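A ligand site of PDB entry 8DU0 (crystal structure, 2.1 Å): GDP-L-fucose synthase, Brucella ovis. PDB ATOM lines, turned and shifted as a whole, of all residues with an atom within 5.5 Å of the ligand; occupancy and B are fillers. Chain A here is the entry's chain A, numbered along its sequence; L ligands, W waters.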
ATOM      1  N   GLY A  32     -12.422   9.440  22.955  1.00  0.00           N
ATOM      2  CA  GLY A  32     -12.686   8.434  21.931  1.00  0.00           C
ATOM      3  C   GLY A  32     -14.094   7.871  21.988  1.00  0.00           C
ATOM      4  O   GLY A  32     -14.287   6.666  21.805  1.00  0.00           O
ATOM      5  N   HIS A  33     -15.084   8.729  22.228  1.00  0.00           N
ATOM      6  CA  HIS A  33     -16.441   8.248  22.452  1.00  0.00           C
ATOM      7  C   HIS A  33     -17.073   7.678  21.183  1.00  0.00           C
ATOM      8  O   HIS A  33     -18.075   6.954  21.284  1.00  0.00           O
ATOM      9  CB  HIS A  33     -17.326   9.354  23.045  1.00  0.00           C
ATOM     10  CG  HIS A  33     -17.636  10.463  22.083  1.00  0.00           C
ATOM     11  ND1 HIS A  33     -16.716  11.404  21.699  1.00  0.00           N
ATOM     12  CD2 HIS A  33     -18.794  10.789  21.446  1.00  0.00           C
ATOM     13  CE1 HIS A  33     -17.273  12.256  20.861  1.00  0.00           C
ATOM     14  NE2 HIS A  33     -18.536  11.905  20.695  1.00  0.00           N
ATOM     15  N   THR A  34     -16.524   7.967  19.996  1.00  0.00           N
ATOM     16  CA  THR A  34     -17.041   7.351  18.784  1.00  0.00           C
ATOM     17  C   THR A  34     -16.493   5.958  18.558  1.00  0.00           C
ATOM     18  O   THR A  34     -17.011   5.224  17.707  1.00  0.00           O
ATOM     19  CB  THR A  34     -16.763   8.234  17.545  1.00  0.00           C
ATOM     20  OG1 THR A  34     -15.345   8.415  17.374  1.00  0.00           O
ATOM     21  CG2 THR A  34     -17.444   9.581  17.670  1.00  0.00           C
ATOM     22  N   GLY A  35     -15.492   5.546  19.337  1.00  0.00           N
ATOM     23  CA  GLY A  35     -14.903   4.236  19.172  1.00  0.00           C
ATOM     24  C   GLY A  35     -15.842   3.134  19.638  1.00  0.00           C
ATOM     25  O   GLY A  35     -16.875   3.351  20.245  1.00  0.00           O
ATOM     26  N   MET A  36     -15.432   1.896  19.342  1.00  0.00           N
ATOM     27  CA  MET A  36     -16.194   0.745  19.778  1.00  0.00           C
ATOM     28  C   MET A  36     -16.244   0.663  21.299  1.00  0.00           C
ATOM     29  O   MET A  36     -17.310   0.437  21.887  1.00  0.00           O
ATOM     30  CB  MET A  36     -15.595  -0.530  19.213  1.00  0.00           C
ATOM     31  CG  MET A  36     -16.536  -1.726  19.284  1.00  0.00           C
ATOM     32  SD  MET A  36     -15.663  -3.235  18.834  1.00  0.00           S
ATOM     33  CE  MET A  36     -16.969  -4.409  19.192  1.00  0.00           C
ATOM     34  N   VAL A  37     -15.087   0.821  21.960  1.00  0.00           N
ATOM     35  CA  VAL A  37     -15.081   0.814  23.423  1.00  0.00           C
ATOM     36  C   VAL A  37     -15.626   2.127  23.969  1.00  0.00           C
ATOM     37  O   VAL A  37     -16.443   2.129  24.891  1.00  0.00           O
ATOM     38  CB  VAL A  37     -13.661   0.526  23.965  1.00  0.00           C
ATOM     39  CG1 VAL A  37     -13.702   0.417  25.477  1.00  0.00           C
ATOM     40  CG2 VAL A  37     -13.098  -0.727  23.365  1.00  0.00           C
ATOM     41  N   GLY A  38     -15.219   3.250  23.378  1.00  0.00           N
ATOM     42  CA  GLY A  38     -15.670   4.550  23.867  1.00  0.00           C
ATOM     43  C   GLY A  38     -17.177   4.707  23.851  1.00  0.00           C
ATOM     44  O   GLY A  38     -17.767   5.248  24.782  1.00  0.00           O
ATOM     45  N   ALA A  56     -15.203  15.323  19.779  1.00  0.00           N
ATOM     46  CA  ALA A  56     -15.043  14.535  18.573  1.00  0.00           C
ATOM     47  C   ALA A  56     -13.591  14.613  18.099  1.00  0.00           C
ATOM     48  O   ALA A  56     -12.864  15.564  18.399  1.00  0.00           O
ATOM     49  CB  ALA A  56     -15.990  15.013  17.478  1.00  0.00           C
ATOM     50  N   HIS A  57     -13.160  13.580  17.377  1.00  0.00           N
ATOM     51  CA  HIS A  57     -11.794  13.574  16.863  1.00  0.00           C
ATOM     52  C   HIS A  57     -11.570  14.756  15.923  1.00  0.00           C
ATOM     53  O   HIS A  57     -10.461  15.298  15.872  1.00  0.00           O
ATOM     54  CB  HIS A  57     -11.512  12.243  16.164  1.00  0.00           C
ATOM     55  CG  HIS A  57     -10.119  12.096  15.632  1.00  0.00           C
ATOM     56  ND1 HIS A  57      -9.781  11.121  14.719  1.00  0.00           N
ATOM     57  CD2 HIS A  57      -8.985  12.784  15.887  1.00  0.00           C
ATOM     58  CE1 HIS A  57      -8.497  11.230  14.427  1.00  0.00           C
ATOM     59  NE2 HIS A  57      -7.992  12.217  15.124  1.00  0.00           N
ATOM     60  N   LEU A  60     -10.793  17.874  18.427  1.00  0.00           N
ATOM     61  CA  LEU A  60      -9.689  17.774  19.379  1.00  0.00           C
ATOM     62  C   LEU A  60      -8.840  16.572  19.018  1.00  0.00           C
ATOM     63  O   LEU A  60      -9.185  15.437  19.360  1.00  0.00           O
ATOM     64  CB  LEU A  60     -10.207  17.667  20.811  1.00  0.00           C
ATOM     65  CG  LEU A  60      -9.143  17.453  21.882  1.00  0.00           C
ATOM     66  CD1 LEU A  60      -8.014  18.501  21.788  1.00  0.00           C
ATOM     67  CD2 LEU A  60      -9.786  17.456  23.258  1.00  0.00           C
ATOM     68  N   ASP A  61      -7.727  16.817  18.330  1.00  0.00           N
ATOM     69  CA  ASP A  61      -6.714  15.787  18.092  1.00  0.00           C
ATOM     70  C   ASP A  61      -5.954  15.563  19.385  1.00  0.00           C
ATOM     71  O   ASP A  61      -5.251  16.463  19.869  1.00  0.00           O
ATOM     72  CB  ASP A  61      -5.785  16.228  16.956  1.00  0.00           C
ATOM     73  CG  ASP A  61      -4.786  15.135  16.536  1.00  0.00           C
ATOM     74  OD1 ASP A  61      -4.510  14.195  17.303  1.00  0.00           O
ATOM     75  OD2 ASP A  61      -4.275  15.234  15.399  1.00  0.00           O
ATOM     76  N   LEU A  62      -6.073  14.367  19.969  1.00  0.00           N
ATOM     77  CA  LEU A  62      -5.519  14.183  21.289  1.00  0.00           C
ATOM     78  C   LEU A  62      -4.009  13.931  21.260  1.00  0.00           C
ATOM     79  O   LEU A  62      -3.406  13.777  22.324  1.00  0.00           O
ATOM     80  CB  LEU A  62      -6.239  13.038  22.003  1.00  0.00           C
ATOM     81  CG  LEU A  62      -7.671  13.359  22.481  1.00  0.00           C
ATOM     82  CD1 LEU A  62      -8.324  12.120  23.054  1.00  0.00           C
ATOM     83  CD2 LEU A  62      -7.643  14.469  23.512  1.00  0.00           C
ATOM     84  N   THR A  63      -3.396  13.894  20.073  1.00  0.00           N
ATOM     85  CA  THR A  63      -1.936  13.886  19.972  1.00  0.00           C
ATOM     86  C   THR A  63      -1.346  15.279  20.123  1.00  0.00           C
ATOM     87  O   THR A  63      -0.125  15.404  20.283  1.00  0.00           O
ATOM     88  CB  THR A  63      -1.474  13.289  18.630  1.00  0.00           C
ATOM     89  OG1 THR A  63      -1.811  14.190  17.563  1.00  0.00           O
ATOM     90  CG2 THR A  63      -2.144  11.950  18.371  1.00  0.00           C
ATOM     91  N   ALA A  83     -10.417   6.086  25.935  1.00  0.00           N
ATOM     92  CA  ALA A  83     -10.725   5.081  24.923  1.00  0.00           C
ATOM     93  C   ALA A  83     -10.339   5.557  23.517  1.00  0.00           C
ATOM     94  O   ALA A  83     -10.704   4.917  22.529  1.00  0.00           O
ATOM     95  CB  ALA A  83     -12.214   4.705  24.972  1.00  0.00           C
ATOM     96  N   ALA A  84      -9.635   6.677  23.421  1.00  0.00           N
ATOM     97  CA  ALA A  84      -9.154   7.143  22.139  1.00  0.00           C
ATOM     98  C   ALA A  84      -7.881   6.394  21.786  1.00  0.00           C
ATOM     99  O   ALA A  84      -7.036   6.144  22.645  1.00  0.00           O
ATOM    100  CB  ALA A  84      -8.907   8.649  22.195  1.00  0.00           C
ATOM    101  N   ALA A  85      -7.762   5.985  20.514  1.00  0.00           N
ATOM    102  CA  ALA A  85      -6.660   5.121  20.122  1.00  0.00           C
ATOM    103  C   ALA A  85      -6.643   4.973  18.615  1.00  0.00           C
ATOM    104  O   ALA A  85      -7.614   5.261  17.930  1.00  0.00           O
ATOM    105  CB  ALA A  85      -6.755   3.730  20.774  1.00  0.00           C
ATOM    106  N   ARG A  86      -5.491   4.512  18.122  1.00  0.00           N
ATOM    107  CA  ARG A  86      -5.359   4.031  16.750  1.00  0.00           C
ATOM    108  C   ARG A  86      -5.185   2.522  16.816  1.00  0.00           C
ATOM    109  O   ARG A  86      -4.196   2.024  17.383  1.00  0.00           O
ATOM    110  CB  ARG A  86      -4.174   4.652  16.026  1.00  0.00           C
ATOM    111  CG  ARG A  86      -4.071   4.116  14.592  1.00  0.00           C
ATOM    112  CD  ARG A  86      -2.736   4.406  13.971  1.00  0.00           C
ATOM    113  NE  ARG A  86      -2.755   5.655  13.227  1.00  0.00           N
ATOM    114  CZ  ARG A  86      -3.263   5.796  12.009  1.00  0.00           C
ATOM    115  NH1 ARG A  86      -3.891   4.796  11.414  1.00  0.00           N
ATOM    116  NH2 ARG A  86      -3.150   6.960  11.382  1.00  0.00           N
ATOM    117  N   VAL A  87      -6.150   1.804  16.251  1.00  0.00           N
ATOM    118  CA  VAL A  87      -6.228   0.355  16.330  1.00  0.00           C
ATOM    119  C   VAL A  87      -6.432  -0.191  14.927  1.00  0.00           C
ATOM    120  O   VAL A  87      -7.003   0.484  14.069  1.00  0.00           O
ATOM    121  CB  VAL A  87      -7.392  -0.078  17.270  1.00  0.00           C
ATOM    122  CG1 VAL A  87      -7.563  -1.579  17.278  1.00  0.00           C
ATOM    123  CG2 VAL A  87      -7.167   0.462  18.680  1.00  0.00           C
ATOM    124  N   ASP A 103       0.590   7.762  17.502  1.00  0.00           N
ATOM    125  CA  ASP A 103      -0.774   8.176  17.853  1.00  0.00           C
ATOM    126  C   ASP A 103      -1.131   7.742  19.263  1.00  0.00           C
ATOM    127  O   ASP A 103      -1.582   8.541  20.082  1.00  0.00           O
ATOM    128  CB  ASP A 103      -1.803   7.596  16.871  1.00  0.00           C
ATOM    129  CG  ASP A 103      -1.757   8.280  15.543  1.00  0.00           C
ATOM    130  OD1 ASP A 103      -0.905   9.189  15.402  1.00  0.00           O
ATOM    131  OD2 ASP A 103      -2.541   7.929  14.640  1.00  0.00           O
ATOM    132  N   ASN A 104      -0.938   6.460  19.558  1.00  0.00           N
ATOM    133  CA  ASN A 104      -1.362   5.975  20.855  1.00  0.00           C
ATOM    134  C   ASN A 104      -0.510   6.530  21.978  1.00  0.00           C
ATOM    135  O   ASN A 104      -1.040   6.837  23.059  1.00  0.00           O
ATOM    136  CB  ASN A 104      -1.346   4.458  20.845  1.00  0.00           C
ATOM    137  CG  ASN A 104      -2.454   3.912  20.003  1.00  0.00           C
ATOM    138  OD1 ASN A 104      -3.629   4.027  20.373  1.00  0.00           O
ATOM    139  ND2 ASN A 104      -2.111   3.358  18.858  1.00  0.00           N
ATOM    140  N   ILE A 107      -1.404  10.292  22.636  1.00  0.00           N
ATOM    141  CA  ILE A 107      -2.707  10.371  23.324  1.00  0.00           C
ATOM    142  C   ILE A 107      -2.524  10.105  24.809  1.00  0.00           C
ATOM    143  O   ILE A 107      -2.965  10.898  25.658  1.00  0.00           O
ATOM    144  CB  ILE A 107      -3.705   9.380  22.704  1.00  0.00           C
ATOM    145  CG1 ILE A 107      -4.157   9.861  21.319  1.00  0.00           C
ATOM    146  CG2 ILE A 107      -4.895   9.158  23.655  1.00  0.00           C
ATOM    147  CD1 ILE A 107      -4.880   8.800  20.513  1.00  0.00           C
ATOM    148  N   LEU A 126      -6.399   2.344  28.738  1.00  0.00           N
ATOM    149  CA  LEU A 126      -6.754   1.032  28.221  1.00  0.00           C
ATOM    150  C   LEU A 126      -5.519   0.385  27.608  1.00  0.00           C
ATOM    151  O   LEU A 126      -4.945   0.916  26.645  1.00  0.00           O
ATOM    152  CB  LEU A 126      -7.884   1.104  27.196  1.00  0.00           C
ATOM    153  CG  LEU A 126      -9.266   1.441  27.742  1.00  0.00           C
ATOM    154  CD1 LEU A 126     -10.284   1.371  26.602  1.00  0.00           C
ATOM    155  CD2 LEU A 126      -9.652   0.535  28.878  1.00  0.00           C
ATOM    156  N   GLY A 127      -5.117  -0.748  28.167  1.00  0.00           N
ATOM    157  CA  GLY A 127      -4.105  -1.589  27.560  1.00  0.00           C
ATOM    158  C   GLY A 127      -4.751  -2.581  26.608  1.00  0.00           C
ATOM    159  O   GLY A 127      -5.769  -2.288  25.958  1.00  0.00           O
ATOM    160  N   SER A 128      -4.150  -3.758  26.523  1.00  0.00           N
ATOM    161  CA  SER A 128      -4.609  -4.722  25.526  1.00  0.00           C
ATOM    162  C   SER A 128      -3.992  -6.073  25.814  1.00  0.00           C
ATOM    163  O   SER A 128      -2.834  -6.162  26.228  1.00  0.00           O
ATOM    164  CB  SER A 128      -4.223  -4.279  24.120  1.00  0.00           C
ATOM    165  OG  SER A 128      -4.689  -5.209  23.177  1.00  0.00           O
ATOM    166  N   SER A 129      -4.753  -7.122  25.533  1.00  0.00           N
ATOM    167  CA  SER A 129      -4.225  -8.474  25.673  1.00  0.00           C
ATOM    168  C   SER A 129      -3.033  -8.724  24.755  1.00  0.00           C
ATOM    169  O   SER A 129      -2.227  -9.615  25.046  1.00  0.00           O
ATOM    170  CB  SER A 129      -5.309  -9.498  25.371  1.00  0.00           C
ATOM    171  OG  SER A 129      -5.831  -9.320  24.070  1.00  0.00           O
ATOM    172  N   CYS A 130      -2.866  -7.972  23.673  1.00  0.00           N
ATOM    173  CA  CYS A 130      -1.794  -8.271  22.740  1.00  0.00           C
ATOM    174  C   CYS A 130      -0.499  -7.544  23.050  1.00  0.00           C
ATOM    175  O   CYS A 130       0.390  -7.500  22.198  1.00  0.00           O
ATOM    176  CB  CYS A 130      -2.242  -7.985  21.307  1.00  0.00           C
ATOM    177  SG  CYS A 130      -3.023  -6.394  21.031  1.00  0.00           S
ATOM    178  N   TYR A 157       2.608  -0.754  18.369  1.00  0.00           N
ATOM    179  CA  TYR A 157       1.415  -0.534  19.180  1.00  0.00           C
ATOM    180  C   TYR A 157       1.640  -0.922  20.643  1.00  0.00           C
ATOM    181  O   TYR A 157       1.288  -0.171  21.571  1.00  0.00           O
ATOM    182  CB  TYR A 157       0.267  -1.331  18.589  1.00  0.00           C
ATOM    183  CG  TYR A 157      -1.051  -1.211  19.302  1.00  0.00           C
ATOM    184  CD1 TYR A 157      -1.887  -0.127  19.101  1.00  0.00           C
ATOM    185  CD2 TYR A 157      -1.505  -2.234  20.131  1.00  0.00           C
ATOM    186  CE1 TYR A 157      -3.117  -0.051  19.713  1.00  0.00           C
ATOM    187  CE2 TYR A 157      -2.729  -2.149  20.756  1.00  0.00           C
ATOM    188  CZ  TYR A 157      -3.546  -1.049  20.529  1.00  0.00           C
ATOM    189  OH  TYR A 157      -4.799  -0.967  21.133  1.00  0.00           O
ATOM    190  N   LYS A 161       1.259   1.373  24.117  1.00  0.00           N
ATOM    191  CA  LYS A 161       0.342   1.039  25.217  1.00  0.00           C
ATOM    192  C   LYS A 161       1.109   0.761  26.512  1.00  0.00           C
ATOM    193  O   LYS A 161       0.638   1.107  27.606  1.00  0.00           O
ATOM    194  CB  LYS A 161      -0.529  -0.168  24.859  1.00  0.00           C
ATOM    195  CG  LYS A 161      -1.553   0.098  23.743  1.00  0.00           C
ATOM    196  CD  LYS A 161      -2.525   1.207  24.146  1.00  0.00           C
ATOM    197  CE  LYS A 161      -3.870   1.105  23.390  1.00  0.00           C
ATOM    198  NZ  LYS A 161      -4.908   1.995  23.993  1.00  0.00           N
ATOM    199  N   MET A 183      -6.663  -4.142  31.187  1.00  0.00           N
ATOM    200  CA  MET A 183      -6.144  -4.972  30.112  1.00  0.00           C
ATOM    201  C   MET A 183      -7.272  -5.839  29.548  1.00  0.00           C
ATOM    202  O   MET A 183      -7.576  -6.911  30.103  1.00  0.00           O
ATOM    203  CB  MET A 183      -4.985  -5.819  30.638  1.00  0.00           C
ATOM    204  CG  MET A 183      -3.838  -4.916  31.214  1.00  0.00           C
ATOM    205  SD  MET A 183      -2.752  -4.208  29.959  1.00  0.00           S
ATOM    206  CE  MET A 183      -1.729  -5.659  29.624  1.00  0.00           C
ATOM    207  N   PRO A 184      -7.931  -5.414  28.485  1.00  0.00           N
ATOM    208  CA  PRO A 184      -9.104  -6.167  27.994  1.00  0.00           C
ATOM    209  C   PRO A 184      -8.696  -7.406  27.231  1.00  0.00           C
ATOM    210  O   PRO A 184      -7.563  -7.877  27.339  1.00  0.00           O
ATOM    211  CB  PRO A 184      -9.830  -5.163  27.095  1.00  0.00           C
ATOM    212  CG  PRO A 184      -9.279  -3.817  27.463  1.00  0.00           C
ATOM    213  CD  PRO A 184      -7.854  -4.079  27.876  1.00  0.00           C
ATOM    214  N   THR A 185      -9.601  -7.940  26.433  1.00  0.00           N
ATOM    215  CA  THR A 185      -9.265  -9.056  25.566  1.00  0.00           C
ATOM    216  C   THR A 185     -10.012  -8.801  24.262  1.00  0.00           C
ATOM    217  O   THR A 185     -10.457  -7.670  24.011  1.00  0.00           O
ATOM    218  CB  THR A 185      -9.572 -10.396  26.270  1.00  0.00           C
ATOM    219  OG1 THR A 185      -9.090 -11.498  25.480  1.00  0.00           O
ATOM    220  CG2 THR A 185     -11.055 -10.539  26.551  1.00  0.00           C
ATOM    221  N   ASN A 186     -10.141  -9.822  23.412  1.00  0.00           N
ATOM    222  CA  ASN A 186     -10.897  -9.660  22.171  1.00  0.00           C
ATOM    223  C   ASN A 186     -12.322  -9.236  22.462  1.00  0.00           C
ATOM    224  O   ASN A 186     -13.026  -9.841  23.283  1.00  0.00           O
ATOM    225  CB  ASN A 186     -10.897 -10.968  21.376  1.00  0.00           C
ATOM    226  CG  ASN A 186      -9.511 -11.374  20.900  1.00  0.00           C
ATOM    227  OD1 ASN A 186      -8.991 -12.424  21.285  1.00  0.00           O
ATOM    228  ND2 ASN A 186      -8.898 -10.522  20.083  1.00  0.00           N
ATOM    229  N   LEU A 187     -12.756  -8.166  21.796  1.00  0.00           N
ATOM    230  CA  LEU A 187     -14.065  -7.587  22.025  1.00  0.00           C
ATOM    231  C   LEU A 187     -14.981  -7.867  20.851  1.00  0.00           C
ATOM    232  O   LEU A 187     -14.532  -7.967  19.708  1.00  0.00           O
ATOM    233  CB  LEU A 187     -13.954  -6.080  22.253  1.00  0.00           C
ATOM    234  CG  LEU A 187     -13.002  -5.632  23.369  1.00  0.00           C
ATOM    235  CD1 LEU A 187     -13.109  -4.155  23.461  1.00  0.00           C
ATOM    236  CD2 LEU A 187     -13.361  -6.262  24.698  1.00  0.00           C
ATOM    237  N   HIS A 200     -11.356  -8.644  12.824  1.00  0.00           N
ATOM    238  CA  HIS A 200     -12.043  -9.272  13.944  1.00  0.00           C
ATOM    239  C   HIS A 200     -12.628 -10.619  13.512  1.00  0.00           C
ATOM    240  O   HIS A 200     -13.415 -10.685  12.562  1.00  0.00           O
ATOM    241  CB  HIS A 200     -13.129  -8.344  14.486  1.00  0.00           C
ATOM    242  CG  HIS A 200     -12.594  -7.118  15.172  1.00  0.00           C
ATOM    243  ND1 HIS A 200     -13.358  -6.334  16.000  1.00  0.00           N
ATOM    244  CD2 HIS A 200     -11.360  -6.552  15.150  1.00  0.00           C
ATOM    245  CE1 HIS A 200     -12.630  -5.339  16.464  1.00  0.00           C
ATOM    246  NE2 HIS A 200     -11.415  -5.438  15.961  1.00  0.00           N
HETATM  247  P1  LIG L   1     -11.717   2.361  17.849  1.00  0.00           P
HETATM  248  O1  LIG L   1     -10.888   2.547  16.634  1.00  0.00           O
HETATM  249  O2  LIG L   1     -13.024   1.635  17.741  1.00  0.00           O
HETATM  250  O3  LIG L   1     -11.965   3.795  18.606  1.00  0.00           O
HETATM  251  C1  LIG L   1     -10.968   4.641  18.282  1.00  0.00           C
HETATM  252  C2  LIG L   1     -11.425   5.949  18.901  1.00  0.00           C
HETATM  253  O4  LIG L   1     -10.337   6.822  19.127  1.00  0.00           O
HETATM  254  C3  LIG L   1     -12.427   6.628  17.910  1.00  0.00           C
HETATM  255  O5  LIG L   1     -13.280   7.457  18.648  1.00  0.00           O
HETATM  256  C4  LIG L   1     -11.484   7.553  17.158  1.00  0.00           C
HETATM  257  O6  LIG L   1     -12.072   8.661  16.730  1.00  0.00           O
HETATM  258  C5  LIG L   1     -10.630   8.005  18.383  1.00  0.00           C
HETATM  259  N1  LIG L   1      -9.376   8.669  17.982  1.00  0.00           N
HETATM  260  C6  LIG L   1      -8.352   8.155  17.163  1.00  0.00           C
HETATM  261  N2  LIG L   1      -7.311   9.035  17.010  1.00  0.00           N
HETATM  262  C7  LIG L   1      -7.689  10.151  17.772  1.00  0.00           C
HETATM  263  C8  LIG L   1      -7.056  11.378  18.023  1.00  0.00           C
HETATM  264  N3  LIG L   1      -5.822  11.692  17.486  1.00  0.00           N
HETATM  265  N4  LIG L   1      -7.638  12.332  18.813  1.00  0.00           N
HETATM  266  C9  LIG L   1      -8.865  11.974  19.324  1.00  0.00           C
HETATM  267  N5  LIG L   1      -9.577  10.860  19.178  1.00  0.00           N
HETATM  268  C10 LIG L   1      -8.973   9.941  18.378  1.00  0.00           C
HETATM  269  O7  LIG L   1     -10.738   1.465  18.826  1.00  0.00           O
HETATM  270  P2  LIG L   1     -11.517   0.425  19.780  1.00  0.00           P
HETATM  271  O8  LIG L   1     -12.523   1.101  20.635  1.00  0.00           O
HETATM  272  O9  LIG L   1     -11.667  -0.936  19.169  1.00  0.00           O
HETATM  273  O10 LIG L   1     -10.222   0.020  20.961  1.00  0.00           O
HETATM  274  C11 LIG L   1      -9.876   1.104  21.758  1.00  0.00           C
HETATM  275  C12 LIG L   1      -8.897   0.587  22.870  1.00  0.00           C
HETATM  276  O11 LIG L   1      -9.540  -0.480  23.632  1.00  0.00           O
HETATM  277  C13 LIG L   1      -7.662  -0.083  22.228  1.00  0.00           C
HETATM  278  O12 LIG L   1      -6.647   0.916  21.969  1.00  0.00           O
HETATM  279  C14 LIG L   1      -7.248  -1.052  23.375  1.00  0.00           C
HETATM  280  O13 LIG L   1      -6.560  -0.428  24.451  1.00  0.00           O
HETATM  281  C15 LIG L   1      -8.654  -1.492  23.933  1.00  0.00           C
HETATM  282  N6  LIG L   1      -9.020  -2.730  23.294  1.00  0.00           N
HETATM  283  C16 LIG L   1      -8.388  -3.877  23.718  1.00  0.00           C
HETATM  284  C17 LIG L   1      -8.527  -5.069  23.083  1.00  0.00           C
HETATM  285  C18 LIG L   1      -7.752  -6.151  23.656  1.00  0.00           C
HETATM  286  O14 LIG L   1      -7.390  -6.190  24.849  1.00  0.00           O
HETATM  287  N7  LIG L   1      -7.353  -7.173  22.811  1.00  0.00           N
HETATM  288  C19 LIG L   1      -9.416  -5.233  21.897  1.00  0.00           C
HETATM  289  C20 LIG L   1     -10.118  -3.959  21.550  1.00  0.00           C
HETATM  290  C21 LIG L   1      -9.918  -2.801  22.215  1.00  0.00           C
HETATM  291  P3  LIG L   1     -12.655   8.636  15.028  1.00  0.00           P
HETATM  292  O15 LIG L   1     -11.607   9.557  14.487  1.00  0.00           O
HETATM  293  O16 LIG L   1     -14.079   9.198  15.188  1.00  0.00           O
HETATM  294  O17 LIG L   1     -12.546   7.171  14.686  1.00  0.00           O
HETATM  295  O   HOH W   1     -11.240   0.691  14.947  1.00  0.00           O
HETATM  296  O   HOH W   2      -6.054  -3.591  21.144  1.00  0.00           O
HETATM  297  O   HOH W   3     -14.792  10.158  19.698  1.00  0.00           O
HETATM  298  O   HOH W   4      -8.571   3.338  15.482  1.00  0.00           O
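O of Gly 127 lies within hydrogen-bond range of O13 of the ligand (2.5 Å). The side-chain hydroxyl (OG) of Ser 129 sits at hydrogen-bond distance from a nitrogen (N7) of the ligand, 2.9 Å away. OG1 of Thr 34 is in hydrogen-bond range of O5 of the ligand, 2.6 Å away. O of Gly 32 sits at hydrogen-bond distance from O5 of the ligand. An oxygen (O14) of the ligand lies within hydrogen-bond range of the backbone NH of Thr 185 (3.2 Å). OD1 of Asp 61 lies within hydrogen-bond range of N3 of the ligand (2.8 Å). The backbone NH (N) of Ala 85 sits at hydrogen-bond distance from an oxygen (O4) of the ligand, at 3.0 Å. The side-chain amino group (NZ) of Lys 161 lies within hydrogen-bond range of an oxygen (O12) of the ligand (2.9 Å). A nitrogen (N4) of the ligand lies within hydrogen-bond range of the backbone NH of Leu 62 (2.8 Å). The backbone NH (N) of Gly 35 sits at hydrogen-bond distance from an oxygen (O5) of the ligand, at 3.0 Å. The backbone carbonyl oxygen (O) of Leu 126 lies within hydrogen-bond range of an oxygen (O13) of the ligand. O12 of the ligand lies within hydrogen-bond range of OH of Tyr 157 (2.8 Å). N of Met 36 lies within hydrogen-bond range of O2 of the ligand (2.9 Å). N of Ser 129 is in hydrogen-bond range of O14 of the ligand. N7 of the ligand lies close to O of Thr 185 (3.4 Å). An oxygen (O14) of the ligand lies close to the side-chain hydroxyl (OG) of Ser 128 (3.3 Å). The backbone NH of Val 37 lies within hydrogen-bond range of an oxygen (O8) of the ligand. A ring nitrogen (ND1) of His 57 sits at hydrogen-bond distance from an oxygen (O15) of the ligand, at 2.4 Å.
Water W4 lies within hydrogen-bond range of O1 of the ligand, N of Val 87 and O of Ala 85. Water W3 lies within hydrogen-bond range of the backbone NH of Thr 34 (2.8 Å), the backbone NH of His 33 (2.9 Å) and an oxygen (O5) of the ligand (3.3 Å). Water W2 lies within hydrogen-bond range of the side-chain hydroxyl of Tyr 157 (2.9 Å) and the side-chain hydroxyl of Ser 128 (2.9 Å).
The backbone NH (N) of Ser 128 sits at hydrogen-bond distance from the side-chain sulfur (SD) of Met 183. The backbone carbonyl oxygen of Pro 184 sits close to the backbone NH of Ser 129 (3.4 Å). The side-chain sulfur (SG) of Cys 130 is in hydrogen-bond range of the side-chain hydroxyl (OG) of Ser 128, at 3.0 Å. The side-chain amino group (NZ) of Lys 161 lies within hydrogen-bond range of the backbone carbonyl oxygen (O) of Leu 126. OG1 of Thr 63 lies within hydrogen-bond range of OD1 of Asp 61 (2.7 Å).
The backbone carbonyl oxygen of Pro 184 sits close to an oxygen (O14) of the ligand. Leu 60 touches the ligand (O to C9, 3.5 Å). CG2 of Thr 63 touches N3 of the ligand, 3.8 Å away. Ala 83 touches the ligand (O to C2, 3.8 Å). CA of Ala 84 touches O4 of the ligand, at 3.3 Å. CG2 of Val 87 touches O12 of the ligand, 3.4 Å away. Asn 186 touches the ligand. Leu 187 touches the ligand (CD1 to C20, 3.6 Å). Hydrophobic or aromatic side chains that line the ligand: Met 36, Val 37, His 57, Leu 62, Ala 84, Ala 85, Val 87, Leu 126, Tyr 157, Pro 184 and Leu 187. Within 4 Å of the ligand: Gly 32, Thr 34, Gly 35, Met 36, Val 37, His 57, Leu 60, Asp 61, Leu 62, Thr 63, Ala 83, Ala 84, Ala 85, Val 87, Leu 126, Gly 127, Ser 128, Ser 129, Tyr 157, Lys 161, Pro 184, Thr 185, Asn 186 and Leu 187. The nearest printed residue that does not touch the ligand is Ile 107 (4.2 Å).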
